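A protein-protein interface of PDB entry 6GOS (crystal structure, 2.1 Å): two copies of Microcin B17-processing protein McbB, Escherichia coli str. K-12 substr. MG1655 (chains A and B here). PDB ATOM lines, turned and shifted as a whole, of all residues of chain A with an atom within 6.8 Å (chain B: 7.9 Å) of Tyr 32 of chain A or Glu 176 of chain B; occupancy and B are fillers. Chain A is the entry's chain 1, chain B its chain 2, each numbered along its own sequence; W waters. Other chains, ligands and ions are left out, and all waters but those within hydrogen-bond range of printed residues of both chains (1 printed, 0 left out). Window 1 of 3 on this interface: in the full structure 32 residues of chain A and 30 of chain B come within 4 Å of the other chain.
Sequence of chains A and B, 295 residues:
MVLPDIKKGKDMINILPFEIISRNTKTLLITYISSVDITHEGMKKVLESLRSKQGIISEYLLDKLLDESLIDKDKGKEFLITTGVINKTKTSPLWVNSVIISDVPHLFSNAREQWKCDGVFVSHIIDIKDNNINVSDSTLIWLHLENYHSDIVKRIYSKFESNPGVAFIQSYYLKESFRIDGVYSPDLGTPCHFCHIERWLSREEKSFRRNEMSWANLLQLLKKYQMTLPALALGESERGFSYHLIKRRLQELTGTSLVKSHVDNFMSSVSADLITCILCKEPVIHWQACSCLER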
ATOM      1  N   LEU A  16       3.888 -21.639  -2.290  1.00  0.00           N
ATOM      2  CA  LEU A  16       4.867 -20.980  -1.426  1.00  0.00           C
ATOM      3  C   LEU A  16       5.789 -22.000  -0.765  1.00  0.00           C
ATOM      4  O   LEU A  16       5.612 -23.216  -0.925  1.00  0.00           O
ATOM      5  CB  LEU A  16       4.168 -20.098  -0.380  1.00  0.00           C
ATOM      6  CG  LEU A  16       3.161 -19.078  -0.949  1.00  0.00           C
ATOM      7  CD1 LEU A  16       2.206 -18.522   0.110  1.00  0.00           C
ATOM      8  CD2 LEU A  16       3.907 -17.943  -1.655  1.00  0.00           C
ATOM      9  N   PRO A  17       6.823 -21.520  -0.080  1.00  0.00           N
ATOM     10  CA  PRO A  17       7.731 -22.487   0.529  1.00  0.00           C
ATOM     11  C   PRO A  17       7.097 -23.174   1.731  1.00  0.00           C
ATOM     12  O   PRO A  17       6.500 -22.506   2.579  1.00  0.00           O
ATOM     13  CB  PRO A  17       8.924 -21.611   0.971  1.00  0.00           C
ATOM     14  CG  PRO A  17       8.881 -20.448   0.014  1.00  0.00           C
ATOM     15  CD  PRO A  17       7.406 -20.163  -0.051  1.00  0.00           C
ATOM     16  N   PHE A  18       7.209 -24.491   1.780  1.00  0.00           N
ATOM     17  CA  PHE A  18       6.719 -25.247   2.921  1.00  0.00           C
ATOM     18  C   PHE A  18       7.326 -26.622   2.909  1.00  0.00           C
ATOM     19  O   PHE A  18       7.872 -27.048   1.897  1.00  0.00           O
ATOM     20  CB  PHE A  18       5.197 -25.325   2.909  1.00  0.00           C
ATOM     21  CG  PHE A  18       4.635 -26.288   1.899  1.00  0.00           C
ATOM     22  CD1 PHE A  18       4.396 -25.891   0.599  1.00  0.00           C
ATOM     23  CD2 PHE A  18       4.303 -27.589   2.271  1.00  0.00           C
ATOM     24  CE1 PHE A  18       3.855 -26.766  -0.323  1.00  0.00           C
ATOM     25  CE2 PHE A  18       3.773 -28.469   1.350  1.00  0.00           C
ATOM     26  CZ  PHE A  18       3.544 -28.054   0.054  1.00  0.00           C
ATOM     27  N   ILE A  30       4.553 -27.116   7.762  1.00  0.00           N
ATOM     28  CA  ILE A  30       5.304 -25.991   8.263  1.00  0.00           C
ATOM     29  C   ILE A  30       5.523 -25.035   7.106  1.00  0.00           C
ATOM     30  O   ILE A  30       6.128 -25.391   6.108  1.00  0.00           O
ATOM     31  CB  ILE A  30       6.668 -26.427   8.810  1.00  0.00           C
ATOM     32  CG1 ILE A  30       6.517 -27.581   9.816  1.00  0.00           C
ATOM     33  CG2 ILE A  30       7.376 -25.235   9.451  1.00  0.00           C
ATOM     34  CD1 ILE A  30       7.840 -28.186  10.250  1.00  0.00           C
ATOM     35  N   THR A  31       5.035 -23.815   7.241  1.00  0.00           N
ATOM     36  CA  THR A  31       5.219 -22.820   6.208  1.00  0.00           C
ATOM     37  C   THR A  31       5.871 -21.601   6.833  1.00  0.00           C
ATOM     38  O   THR A  31       6.181 -21.582   8.017  1.00  0.00           O
ATOM     39  CB  THR A  31       3.885 -22.441   5.533  1.00  0.00           C
ATOM     40  OG1 THR A  31       3.207 -21.436   6.300  1.00  0.00           O
ATOM     41  CG2 THR A  31       2.988 -23.663   5.378  1.00  0.00           C
ATOM     42  N   TYR A  32       6.063 -20.573   6.022  1.00  0.00           N
ATOM     43  CA  TYR A  32       6.571 -19.320   6.526  1.00  0.00           C
ATOM     44  C   TYR A  32       5.555 -18.635   7.423  1.00  0.00           C
ATOM     45  O   TYR A  32       5.933 -17.769   8.216  1.00  0.00           O
ATOM     46  CB  TYR A  32       6.996 -18.411   5.362  1.00  0.00           C
ATOM     47  CG  TYR A  32       8.333 -18.777   4.693  1.00  0.00           C
ATOM     48  CD1 TYR A  32       9.208 -19.748   5.229  1.00  0.00           C
ATOM     49  CD2 TYR A  32       8.760 -18.098   3.557  1.00  0.00           C
ATOM     50  CE1 TYR A  32      10.419 -20.052   4.612  1.00  0.00           C
ATOM     51  CE2 TYR A  32       9.976 -18.401   2.946  1.00  0.00           C
ATOM     52  CZ  TYR A  32      10.794 -19.366   3.477  1.00  0.00           C
ATOM     53  OH  TYR A  32      11.996 -19.626   2.878  1.00  0.00           O
ATOM     54  N   ILE A  33       4.283 -19.014   7.296  1.00  0.00           N
ATOM     55  CA  ILE A  33       3.177 -18.356   7.977  1.00  0.00           C
ATOM     56  C   ILE A  33       2.710 -19.136   9.205  1.00  0.00           C
ATOM     57  O   ILE A  33       2.374 -18.535  10.245  1.00  0.00           O
ATOM     58  CB  ILE A  33       1.986 -18.171   7.007  1.00  0.00           C
ATOM     59  CG1 ILE A  33       2.412 -17.389   5.760  1.00  0.00           C
ATOM     60  CG2 ILE A  33       0.815 -17.463   7.681  1.00  0.00           C
ATOM     61  CD1 ILE A  33       2.708 -15.918   5.996  1.00  0.00           C
ATOM     62  N   SER A  34       2.680 -20.456   9.111  1.00  0.00           N
ATOM     63  CA  SER A  34       2.078 -21.251  10.157  1.00  0.00           C
ATOM     64  C   SER A  34       2.630 -22.663  10.207  1.00  0.00           C
ATOM     65  O   SER A  34       3.391 -23.085   9.334  1.00  0.00           O
ATOM     66  CB  SER A  34       0.556 -21.316   9.940  1.00  0.00           C
ATOM     67  OG  SER A  34       0.244 -22.196   8.858  1.00  0.00           O
ATOM     68  N   THR A  83      -3.017 -20.808   5.701  1.00  0.00           N
ATOM     69  CA  THR A  83      -1.845 -21.428   6.339  1.00  0.00           C
ATOM     70  C   THR A  83      -0.507 -21.065   5.694  1.00  0.00           C
ATOM     71  O   THR A  83       0.534 -21.311   6.299  1.00  0.00           O
ATOM     72  CB  THR A  83      -1.951 -22.971   6.434  1.00  0.00           C
ATOM     73  OG1 THR A  83      -2.110 -23.551   5.124  1.00  0.00           O
ATOM     74  CG2 THR A  83      -3.114 -23.373   7.340  1.00  0.00           C
ATOM     75  N   GLY A  84      -0.530 -20.501   4.487  1.00  0.00           N
ATOM     76  CA  GLY A  84       0.688 -20.068   3.775  1.00  0.00           C
ATOM     77  C   GLY A  84       1.296 -21.082   2.809  1.00  0.00           C
ATOM     78  O   GLY A  84       2.502 -21.048   2.531  1.00  0.00           O
ATOM     79  N   ARG A 248      16.740 -13.929  -6.109  1.00  0.00           N
ATOM     80  CA  ARG A 248      15.840 -13.179  -5.229  1.00  0.00           C
ATOM     81  C   ARG A 248      15.395 -11.848  -5.791  1.00  0.00           C
ATOM     82  O   ARG A 248      14.231 -11.440  -5.594  1.00  0.00           O
ATOM     83  CB  ARG A 248      16.450 -12.972  -3.856  1.00  0.00           C
ATOM     84  CG  ARG A 248      16.525 -14.244  -3.040  1.00  0.00           C
ATOM     85  CD  ARG A 248      15.167 -14.945  -2.927  1.00  0.00           C
ATOM     86  NE  ARG A 248      15.141 -15.812  -1.757  1.00  0.00           N
ATOM     87  CZ  ARG A 248      14.304 -16.827  -1.582  1.00  0.00           C
ATOM     88  NH1 ARG A 248      13.411 -17.141  -2.508  1.00  0.00           N
ATOM     89  NH2 ARG A 248      14.360 -17.537  -0.456  1.00  0.00           N
ATOM     90  N   LEU A 258       7.358 -12.965  -1.927  1.00  0.00           N
ATOM     91  CA  LEU A 258       7.258 -13.452  -0.547  1.00  0.00           C
ATOM     92  C   LEU A 258       7.224 -12.314   0.492  1.00  0.00           C
ATOM     93  O   LEU A 258       6.513 -12.403   1.495  1.00  0.00           O
ATOM     94  CB  LEU A 258       8.416 -14.406  -0.264  1.00  0.00           C
ATOM     95  CG  LEU A 258       8.398 -15.685  -1.107  1.00  0.00           C
ATOM     96  CD1 LEU A 258       9.682 -16.472  -0.894  1.00  0.00           C
ATOM     97  CD2 LEU A 258       7.193 -16.523  -0.757  1.00  0.00           C
ATOM     98  N   VAL A 259       8.009 -11.264   0.249  1.00  0.00           N
ATOM     99  CA  VAL A 259       8.056 -10.073   1.084  1.00  0.00           C
ATOM    100  C   VAL A 259       7.948  -8.891   0.125  1.00  0.00           C
ATOM    101  O   VAL A 259       8.744  -8.774  -0.789  1.00  0.00           O
ATOM    102  CB  VAL A 259       9.389 -10.015   1.869  1.00  0.00           C
ATOM    103  CG1 VAL A 259       9.610  -8.653   2.526  1.00  0.00           C
ATOM    104  CG2 VAL A 259       9.417 -11.110   2.940  1.00  0.00           C
ATOM    105  N   TYR B 173      18.586 -23.973  10.273  1.00  0.00           N
ATOM    106  CA  TYR B 173      17.524 -23.220   9.622  1.00  0.00           C
ATOM    107  C   TYR B 173      16.279 -23.124  10.508  1.00  0.00           C
ATOM    108  O   TYR B 173      15.811 -24.119  11.079  1.00  0.00           O
ATOM    109  CB  TYR B 173      17.235 -23.837   8.227  1.00  0.00           C
ATOM    110  CG  TYR B 173      18.440 -23.764   7.262  1.00  0.00           C
ATOM    111  CD1 TYR B 173      19.404 -24.769   7.249  1.00  0.00           C
ATOM    112  CD2 TYR B 173      18.622 -22.677   6.393  1.00  0.00           C
ATOM    113  CE1 TYR B 173      20.487 -24.707   6.388  1.00  0.00           C
ATOM    114  CE2 TYR B 173      19.714 -22.605   5.527  1.00  0.00           C
ATOM    115  CZ  TYR B 173      20.644 -23.631   5.538  1.00  0.00           C
ATOM    116  OH  TYR B 173      21.729 -23.620   4.717  1.00  0.00           O
ATOM    117  N   LEU B 174      15.795 -21.901  10.660  1.00  0.00           N
ATOM    118  CA  LEU B 174      14.629 -21.592  11.472  1.00  0.00           C
ATOM    119  C   LEU B 174      13.695 -20.801  10.605  1.00  0.00           C
ATOM    120  O   LEU B 174      13.809 -19.579  10.505  1.00  0.00           O
ATOM    121  CB  LEU B 174      15.016 -20.776  12.701  1.00  0.00           C
ATOM    122  CG  LEU B 174      15.884 -21.507  13.728  1.00  0.00           C
ATOM    123  CD1 LEU B 174      16.486 -20.501  14.707  1.00  0.00           C
ATOM    124  CD2 LEU B 174      15.106 -22.599  14.429  1.00  0.00           C
ATOM    125  N   LYS B 175      12.824 -21.526   9.920  1.00  0.00           N
ATOM    126  CA  LYS B 175      11.782 -20.950   9.081  1.00  0.00           C
ATOM    127  C   LYS B 175      12.449 -20.236   7.870  1.00  0.00           C
ATOM    128  O   LYS B 175      13.095 -20.917   7.079  1.00  0.00           O
ATOM    129  CB  LYS B 175      10.816 -20.100   9.939  1.00  0.00           C
ATOM    130  CG  LYS B 175       9.440 -19.950   9.337  1.00  0.00           C
ATOM    131  CD  LYS B 175       8.343 -19.744  10.384  1.00  0.00           C
ATOM    132  CE  LYS B 175       8.440 -18.391  11.072  1.00  0.00           C
ATOM    133  NZ  LYS B 175       8.179 -17.258  10.139  1.00  0.00           N
ATOM    134  N   GLU B 176      12.343 -18.913   7.730  1.00  0.00           N
ATOM    135  CA  GLU B 176      13.003 -18.219   6.591  1.00  0.00           C
ATOM    136  C   GLU B 176      14.457 -17.809   6.887  1.00  0.00           C
ATOM    137  O   GLU B 176      15.114 -17.302   6.007  1.00  0.00           O
ATOM    138  CB  GLU B 176      12.204 -17.002   6.100  1.00  0.00           C
ATOM    139  CG  GLU B 176      11.963 -15.926   7.130  1.00  0.00           C
ATOM    140  CD  GLU B 176      10.713 -16.201   7.960  1.00  0.00           C
ATOM    141  OE1 GLU B 176       9.592 -15.871   7.509  1.00  0.00           O
ATOM    142  OE2 GLU B 176      10.839 -16.759   9.065  1.00  0.00           O
ATOM    143  N   SER B 177      14.936 -18.044   8.110  1.00  0.00           N
ATOM    144  CA  SER B 177      16.268 -17.648   8.520  1.00  0.00           C
ATOM    145  C   SER B 177      17.247 -18.779   8.499  1.00  0.00           C
ATOM    146  O   SER B 177      16.892 -19.911   8.810  1.00  0.00           O
ATOM    147  CB  SER B 177      16.236 -17.105   9.927  1.00  0.00           C
ATOM    148  OG  SER B 177      15.507 -15.915   9.928  1.00  0.00           O
ATOM    149  N   PHE B 178      18.482 -18.452   8.109  1.00  0.00           N
ATOM    150  CA  PHE B 178      19.662 -19.265   8.384  1.00  0.00           C
ATOM    151  C   PHE B 178      20.359 -18.631   9.607  1.00  0.00           C
ATOM    152  O   PHE B 178      20.717 -17.456   9.553  1.00  0.00           O
ATOM    153  CB  PHE B 178      20.549 -19.292   7.136  1.00  0.00           C
ATOM    154  CG  PHE B 178      21.845 -20.056   7.292  1.00  0.00           C
ATOM    155  CD1 PHE B 178      21.863 -21.337   7.829  1.00  0.00           C
ATOM    156  CD2 PHE B 178      23.055 -19.482   6.879  1.00  0.00           C
ATOM    157  CE1 PHE B 178      23.046 -22.052   7.934  1.00  0.00           C
ATOM    158  CE2 PHE B 178      24.238 -20.178   7.012  1.00  0.00           C
ATOM    159  CZ  PHE B 178      24.240 -21.474   7.530  1.00  0.00           C
ATOM    160  N   ARG B 179      20.477 -19.380  10.721  1.00  0.00           N
ATOM    161  CA  ARG B 179      21.148 -18.884  11.937  1.00  0.00           C
ATOM    162  C   ARG B 179      22.511 -19.528  12.121  1.00  0.00           C
ATOM    163  O   ARG B 179      22.629 -20.752  12.046  1.00  0.00           O
ATOM    164  CB  ARG B 179      20.334 -19.133  13.216  1.00  0.00           C
ATOM    165  CG  ARG B 179      20.984 -18.498  14.474  1.00  0.00           C
ATOM    166  CD  ARG B 179      20.308 -18.876  15.773  1.00  0.00           C
ATOM    167  NE  ARG B 179      21.022 -18.376  16.959  1.00  0.00           N
ATOM    168  CZ  ARG B 179      20.850 -17.181  17.546  1.00  0.00           C
ATOM    169  NH1 ARG B 179      19.985 -16.268  17.072  1.00  0.00           N
ATOM    170  NH2 ARG B 179      21.585 -16.874  18.613  1.00  0.00           N
ATOM    171  N   TRP B 215       5.634 -20.429  18.139  1.00  0.00           N
ATOM    172  CA  TRP B 215       6.505 -21.358  17.439  1.00  0.00           C
ATOM    173  C   TRP B 215       7.134 -22.404  18.382  1.00  0.00           C
ATOM    174  O   TRP B 215       7.543 -23.475  17.924  1.00  0.00           O
ATOM    175  CB  TRP B 215       7.556 -20.608  16.558  1.00  0.00           C
ATOM    176  CG  TRP B 215       6.836 -20.071  15.380  1.00  0.00           C
ATOM    177  CD1 TRP B 215       6.163 -18.874  15.314  1.00  0.00           C
ATOM    178  CD2 TRP B 215       6.563 -20.753  14.136  1.00  0.00           C
ATOM    179  NE1 TRP B 215       5.538 -18.749  14.095  1.00  0.00           N
ATOM    180  CE2 TRP B 215       5.743 -19.889  13.358  1.00  0.00           C
ATOM    181  CE3 TRP B 215       6.944 -21.993  13.598  1.00  0.00           C
ATOM    182  CZ2 TRP B 215       5.285 -20.231  12.061  1.00  0.00           C
ATOM    183  CZ3 TRP B 215       6.494 -22.338  12.284  1.00  0.00           C
ATOM    184  CH2 TRP B 215       5.682 -21.446  11.534  1.00  0.00           C
ATOM    185  N   ALA B 231      14.691 -27.606   7.228  1.00  0.00           N
ATOM    186  CA  ALA B 231      14.828 -26.342   6.523  1.00  0.00           C
ATOM    187  C   ALA B 231      13.731 -26.314   5.472  1.00  0.00           C
ATOM    188  O   ALA B 231      13.430 -27.353   4.836  1.00  0.00           O
ATOM    189  CB  ALA B 231      16.197 -26.242   5.880  1.00  0.00           C
ATOM    190  N   LEU B 232      13.125 -25.150   5.294  1.00  0.00           N
ATOM    191  CA  LEU B 232      11.966 -25.030   4.411  1.00  0.00           C
ATOM    192  C   LEU B 232      12.368 -24.811   2.959  1.00  0.00           C
ATOM    193  O   LEU B 232      12.853 -23.736   2.606  1.00  0.00           O
ATOM    194  CB  LEU B 232      11.024 -23.915   4.888  1.00  0.00           C
ATOM    195  CG  LEU B 232       9.887 -24.372   5.806  1.00  0.00           C
ATOM    196  CD1 LEU B 232      10.347 -25.348   6.881  1.00  0.00           C
ATOM    197  CD2 LEU B 232       9.216 -23.152   6.405  1.00  0.00           C
ATOM    198  N   ALA B 233      12.182 -25.847   2.139  1.00  0.00           N
ATOM    199  CA  ALA B 233      12.280 -25.739   0.688  1.00  0.00           C
ATOM    200  C   ALA B 233      13.578 -25.065   0.200  1.00  0.00           C
ATOM    201  O   ALA B 233      13.548 -24.170  -0.642  1.00  0.00           O
ATOM    202  CB  ALA B 233      11.052 -24.994   0.158  1.00  0.00           C
ATOM    203  N   LEU B 234      14.705 -25.504   0.743  1.00  0.00           N
ATOM    204  CA  LEU B 234      16.007 -25.055   0.264  1.00  0.00           C
ATOM    205  C   LEU B 234      16.251 -25.549  -1.144  1.00  0.00           C
ATOM    206  O   LEU B 234      15.953 -26.689  -1.446  1.00  0.00           O
ATOM    207  CB  LEU B 234      17.127 -25.593   1.134  1.00  0.00           C
ATOM    208  CG  LEU B 234      17.231 -25.101   2.556  1.00  0.00           C
ATOM    209  CD1 LEU B 234      18.472 -25.725   3.177  1.00  0.00           C
ATOM    210  CD2 LEU B 234      17.272 -23.585   2.627  1.00  0.00           C
ATOM    211  N   GLU B 238      19.870 -21.067  -2.112  1.00  0.00           N
ATOM    212  CA  GLU B 238      19.898 -20.930  -0.670  1.00  0.00           C
ATOM    213  C   GLU B 238      21.121 -21.636  -0.082  1.00  0.00           C
ATOM    214  O   GLU B 238      21.763 -21.113   0.818  1.00  0.00           O
ATOM    215  CB  GLU B 238      18.637 -21.478  -0.030  1.00  0.00           C
ATOM    216  CG  GLU B 238      17.392 -20.641  -0.279  1.00  0.00           C
ATOM    217  CD  GLU B 238      16.763 -20.857  -1.645  1.00  0.00           C
ATOM    218  OE1 GLU B 238      16.973 -21.927  -2.268  1.00  0.00           O
ATOM    219  OE2 GLU B 238      16.059 -19.937  -2.102  1.00  0.00           O
ATOM    220  N   PHE B 241      24.276 -19.546  -1.010  1.00  0.00           N
ATOM    221  CA  PHE B 241      24.284 -18.432  -0.070  1.00  0.00           C
ATOM    222  C   PHE B 241      24.781 -18.844   1.328  1.00  0.00           C
ATOM    223  O   PHE B 241      25.620 -18.162   1.943  1.00  0.00           O
ATOM    224  CB  PHE B 241      22.867 -17.866  -0.022  1.00  0.00           C
ATOM    225  CG  PHE B 241      22.681 -16.669   0.858  1.00  0.00           C
ATOM    226  CD1 PHE B 241      22.999 -15.400   0.409  1.00  0.00           C
ATOM    227  CD2 PHE B 241      22.071 -16.798   2.075  1.00  0.00           C
ATOM    228  CE1 PHE B 241      22.763 -14.297   1.194  1.00  0.00           C
ATOM    229  CE2 PHE B 241      21.814 -15.693   2.850  1.00  0.00           C
ATOM    230  CZ  PHE B 241      22.173 -14.451   2.422  1.00  0.00           C
ATOM    231  N   SER B 271      22.330 -14.052  11.870  1.00  0.00           N
ATOM    232  CA  SER B 271      21.110 -14.555  11.274  1.00  0.00           C
ATOM    233  C   SER B 271      20.909 -13.906   9.913  1.00  0.00           C
ATOM    234  O   SER B 271      21.021 -12.686   9.790  1.00  0.00           O
ATOM    235  CB  SER B 271      19.919 -14.278  12.203  1.00  0.00           C
ATOM    236  OG  SER B 271      20.087 -15.019  13.421  1.00  0.00           O
ATOM    237  N   ALA B 272      20.615 -14.723   8.900  1.00  0.00           N
ATOM    238  CA  ALA B 272      20.388 -14.250   7.522  1.00  0.00           C
ATOM    239  C   ALA B 272      18.970 -14.617   7.088  1.00  0.00           C
ATOM    240  O   ALA B 272      18.623 -15.798   7.041  1.00  0.00           O
ATOM    241  CB  ALA B 272      21.398 -14.876   6.569  1.00  0.00           C
ATOM    242  N   ASP B 273      18.162 -13.614   6.789  1.00  0.00           N
ATOM    243  CA  ASP B 273      16.879 -13.829   6.131  1.00  0.00           C
ATOM    244  C   ASP B 273      17.139 -14.296   4.688  1.00  0.00           C
ATOM    245  O   ASP B 273      17.760 -13.588   3.897  1.00  0.00           O
ATOM    246  CB  ASP B 273      16.069 -12.543   6.159  1.00  0.00           C
ATOM    247  CG  ASP B 273      14.679 -12.706   5.566  1.00  0.00           C
ATOM    248  OD1 ASP B 273      14.549 -13.279   4.477  1.00  0.00           O
ATOM    249  OD2 ASP B 273      13.709 -12.240   6.179  1.00  0.00           O
ATOM    250  N   LEU B 274      16.683 -15.496   4.356  1.00  0.00           N
ATOM    251  CA  LEU B 274      16.957 -16.105   3.061  1.00  0.00           C
ATOM    252  C   LEU B 274      16.160 -15.503   1.904  1.00  0.00           C
ATOM    253  O   LEU B 274      16.488 -15.755   0.751  1.00  0.00           O
ATOM    254  CB  LEU B 274      16.716 -17.619   3.114  1.00  0.00           C
ATOM    255  CG  LEU B 274      17.640 -18.465   3.967  1.00  0.00           C
ATOM    256  CD1 LEU B 274      17.166 -19.917   3.992  1.00  0.00           C
ATOM    257  CD2 LEU B 274      19.057 -18.387   3.461  1.00  0.00           C
ATOM    258  N   ILE B 275      15.145 -14.702   2.218  1.00  0.00           N
ATOM    259  CA  ILE B 275      14.323 -14.025   1.246  1.00  0.00           C
ATOM    260  C   ILE B 275      14.956 -12.640   0.897  1.00  0.00           C
ATOM    261  O   ILE B 275      15.283 -12.371  -0.266  1.00  0.00           O
ATOM    262  CB  ILE B 275      12.875 -13.798   1.782  1.00  0.00           C
ATOM    263  CG1 ILE B 275      12.217 -15.123   2.274  1.00  0.00           C
ATOM    264  CG2 ILE B 275      12.037 -13.075   0.715  1.00  0.00           C
ATOM    265  CD1 ILE B 275      10.965 -14.947   3.129  1.00  0.00           C
ATOM    266  N   THR B 276      15.087 -11.767   1.900  1.00  0.00           N
ATOM    267  CA  THR B 276      15.663 -10.423   1.708  1.00  0.00           C
ATOM    268  C   THR B 276      17.197 -10.438   1.588  1.00  0.00           C
ATOM    269  O   THR B 276      17.783  -9.445   1.202  1.00  0.00           O
ATOM    270  CB  THR B 276      15.355  -9.519   2.888  1.00  0.00           C
ATOM    271  OG1 THR B 276      15.937 -10.084   4.055  1.00  0.00           O
ATOM    272  CG2 THR B 276      13.853  -9.347   3.102  1.00  0.00           C
ATOM    273  N   CYS B 277      17.823 -11.551   1.962  1.00  0.00           N
ATOM    274  CA  CYS B 277      19.276 -11.707   2.051  1.00  0.00           C
ATOM    275  C   CYS B 277      19.921 -10.751   3.059  1.00  0.00           C
ATOM    276  O   CYS B 277      21.121 -10.535   2.993  1.00  0.00           O
ATOM    277  CB  CYS B 277      19.945 -11.598   0.678  1.00  0.00           C
ATOM    278  SG  CYS B 277      19.242 -12.706  -0.560  1.00  0.00           S
ATOM    279  N   ILE B 278      19.144 -10.234   4.016  1.00  0.00           N
ATOM    280  CA  ILE B 278      19.637  -9.274   4.995  1.00  0.00           C
ATOM    281  C   ILE B 278      20.221 -10.025   6.208  1.00  0.00           C
ATOM    282  O   ILE B 278      19.592 -10.950   6.729  1.00  0.00           O
ATOM    283  CB  ILE B 278      18.521  -8.268   5.387  1.00  0.00           C
ATOM    284  CG1 ILE B 278      18.267  -7.316   4.203  1.00  0.00           C
ATOM    285  CG2 ILE B 278      18.890  -7.443   6.618  1.00  0.00           C
ATOM    286  CD1 ILE B 278      17.047  -6.424   4.362  1.00  0.00           C
HETATM  287  O   HOH W   1      13.722 -21.559   4.051  1.00  0.00           O
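The backbone carbonyl oxygen of Tyr 32 of chain A is in hydrogen-bond range of the side-chain amino group of Lys 175 of chain B (3.0 Å).
OE2 of Glu 238 of chain B is in salt-bridge range of NH2 of Arg 248 of chain A, 3.4 Å away.
The backbone carbonyl oxygen of Leu 274 of chain B lies within hydrogen-bond range of the guanidinium group of Arg 248 of chain A.
Water W1 lies within hydrogen-bond range of O of Leu 232 of chain B (2.8 Å), OH of Tyr 32 of chain A (2.8 Å) and O of Lys 175 of chain B (3.2 Å).
Of chain A, only Tyr 32 (3.7 Å) comes within 4 Å of Glu 176 of chain B.
Of the printed residues of chain B, Val 259 of chain A touches Ile 275.
Of the printed residues of chain B, Thr 31 of chain A touches Lys 175, Trp 215 and Leu 232.
Printed residues of chain B within 4 Å of Arg 248 of chain A: Glu 238, Leu 274, Ile 275 and Cys 277.
The backbone NH (N) of Ile 33 of chain A is in hydrogen-bond range of the side-chain hydroxyl (OG1) of Thr 31 of chain A.
The backbone NH (N) of Ser 34 of chain A sits at hydrogen-bond distance from the side-chain hydroxyl (OG1) of Thr 31 of chain A, at 3.0 Å.
The side-chain hydroxyl (OG1) of Thr 31 of chain A sits at hydrogen-bond distance from the backbone carbonyl oxygen (O) of Thr 83 of chain A.
NZ of Lys 175 of chain B is in salt-bridge range of OE2 of Glu 176 of chain B (2.9 Å).
The backbone carbonyl oxygen of Glu 176 of chain B sits at hydrogen-bond distance from the backbone NH of Leu 274 of chain B.
The side-chain carboxylate (OD1) of Asp 273 of chain B is in hydrogen-bond range of the backbone NH (N) of Ile 275 of chain B, at 2.7 Å.
No position is printed for both chains.
Leu 232 of chain B touches Ile 30 of chain A (CD2 to O, 3.8 Å).
Thr 31 of chain A touches Trp 215 of chain B.
C of Thr 31 of chain A touches CD2 of Leu 232 of chain B, at 3.7 Å.
Tyr 32 of chain A touches Ile 275 of chain B (CE2 to CD1, 3.6 Å).
Ile 33 of chain A touches Trp 215 of chain B (O to CZ2, 3.8 Å).
Trp 215 of chain B touches Ser 34 of chain A.
Arg 248 of chain A touches Ile 275 of chain B (CG to O, 3.6 Å).
CG of Arg 248 of chain A touches SG of Cys 277 of chain B, 3.99 Å away.
Ile 275 of chain B touches Leu 258 of chain A.
Val 259 of chain A touches Ile 275 of chain B (CG2 to CG2, 3.96 Å).
Hydrophobic or aromatic side chains of chain A within 4 Å of the printed part of chain B: Ile 30, Tyr 32, Leu 258 and Val 259.
Printed residues of chain B that touch a printed residue of chain A: Lys 175, Glu 176, Trp 215, Leu 232, Glu 238, Leu 274, Ile 275 and Cys 277.
Hydrophobic or aromatic side chains of chain B within 4 Å of the printed part of chain A: Trp 215, Leu 232 and Ile 275.
Among the printed residues, 16 pairs touch across the chains.
Among the printed residues, Asp or Glu carboxylates within 4 Å of a Lys or Arg side-chain nitrogen of the other chain: Arg 248 of chain A with Glu 238 of chain B.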
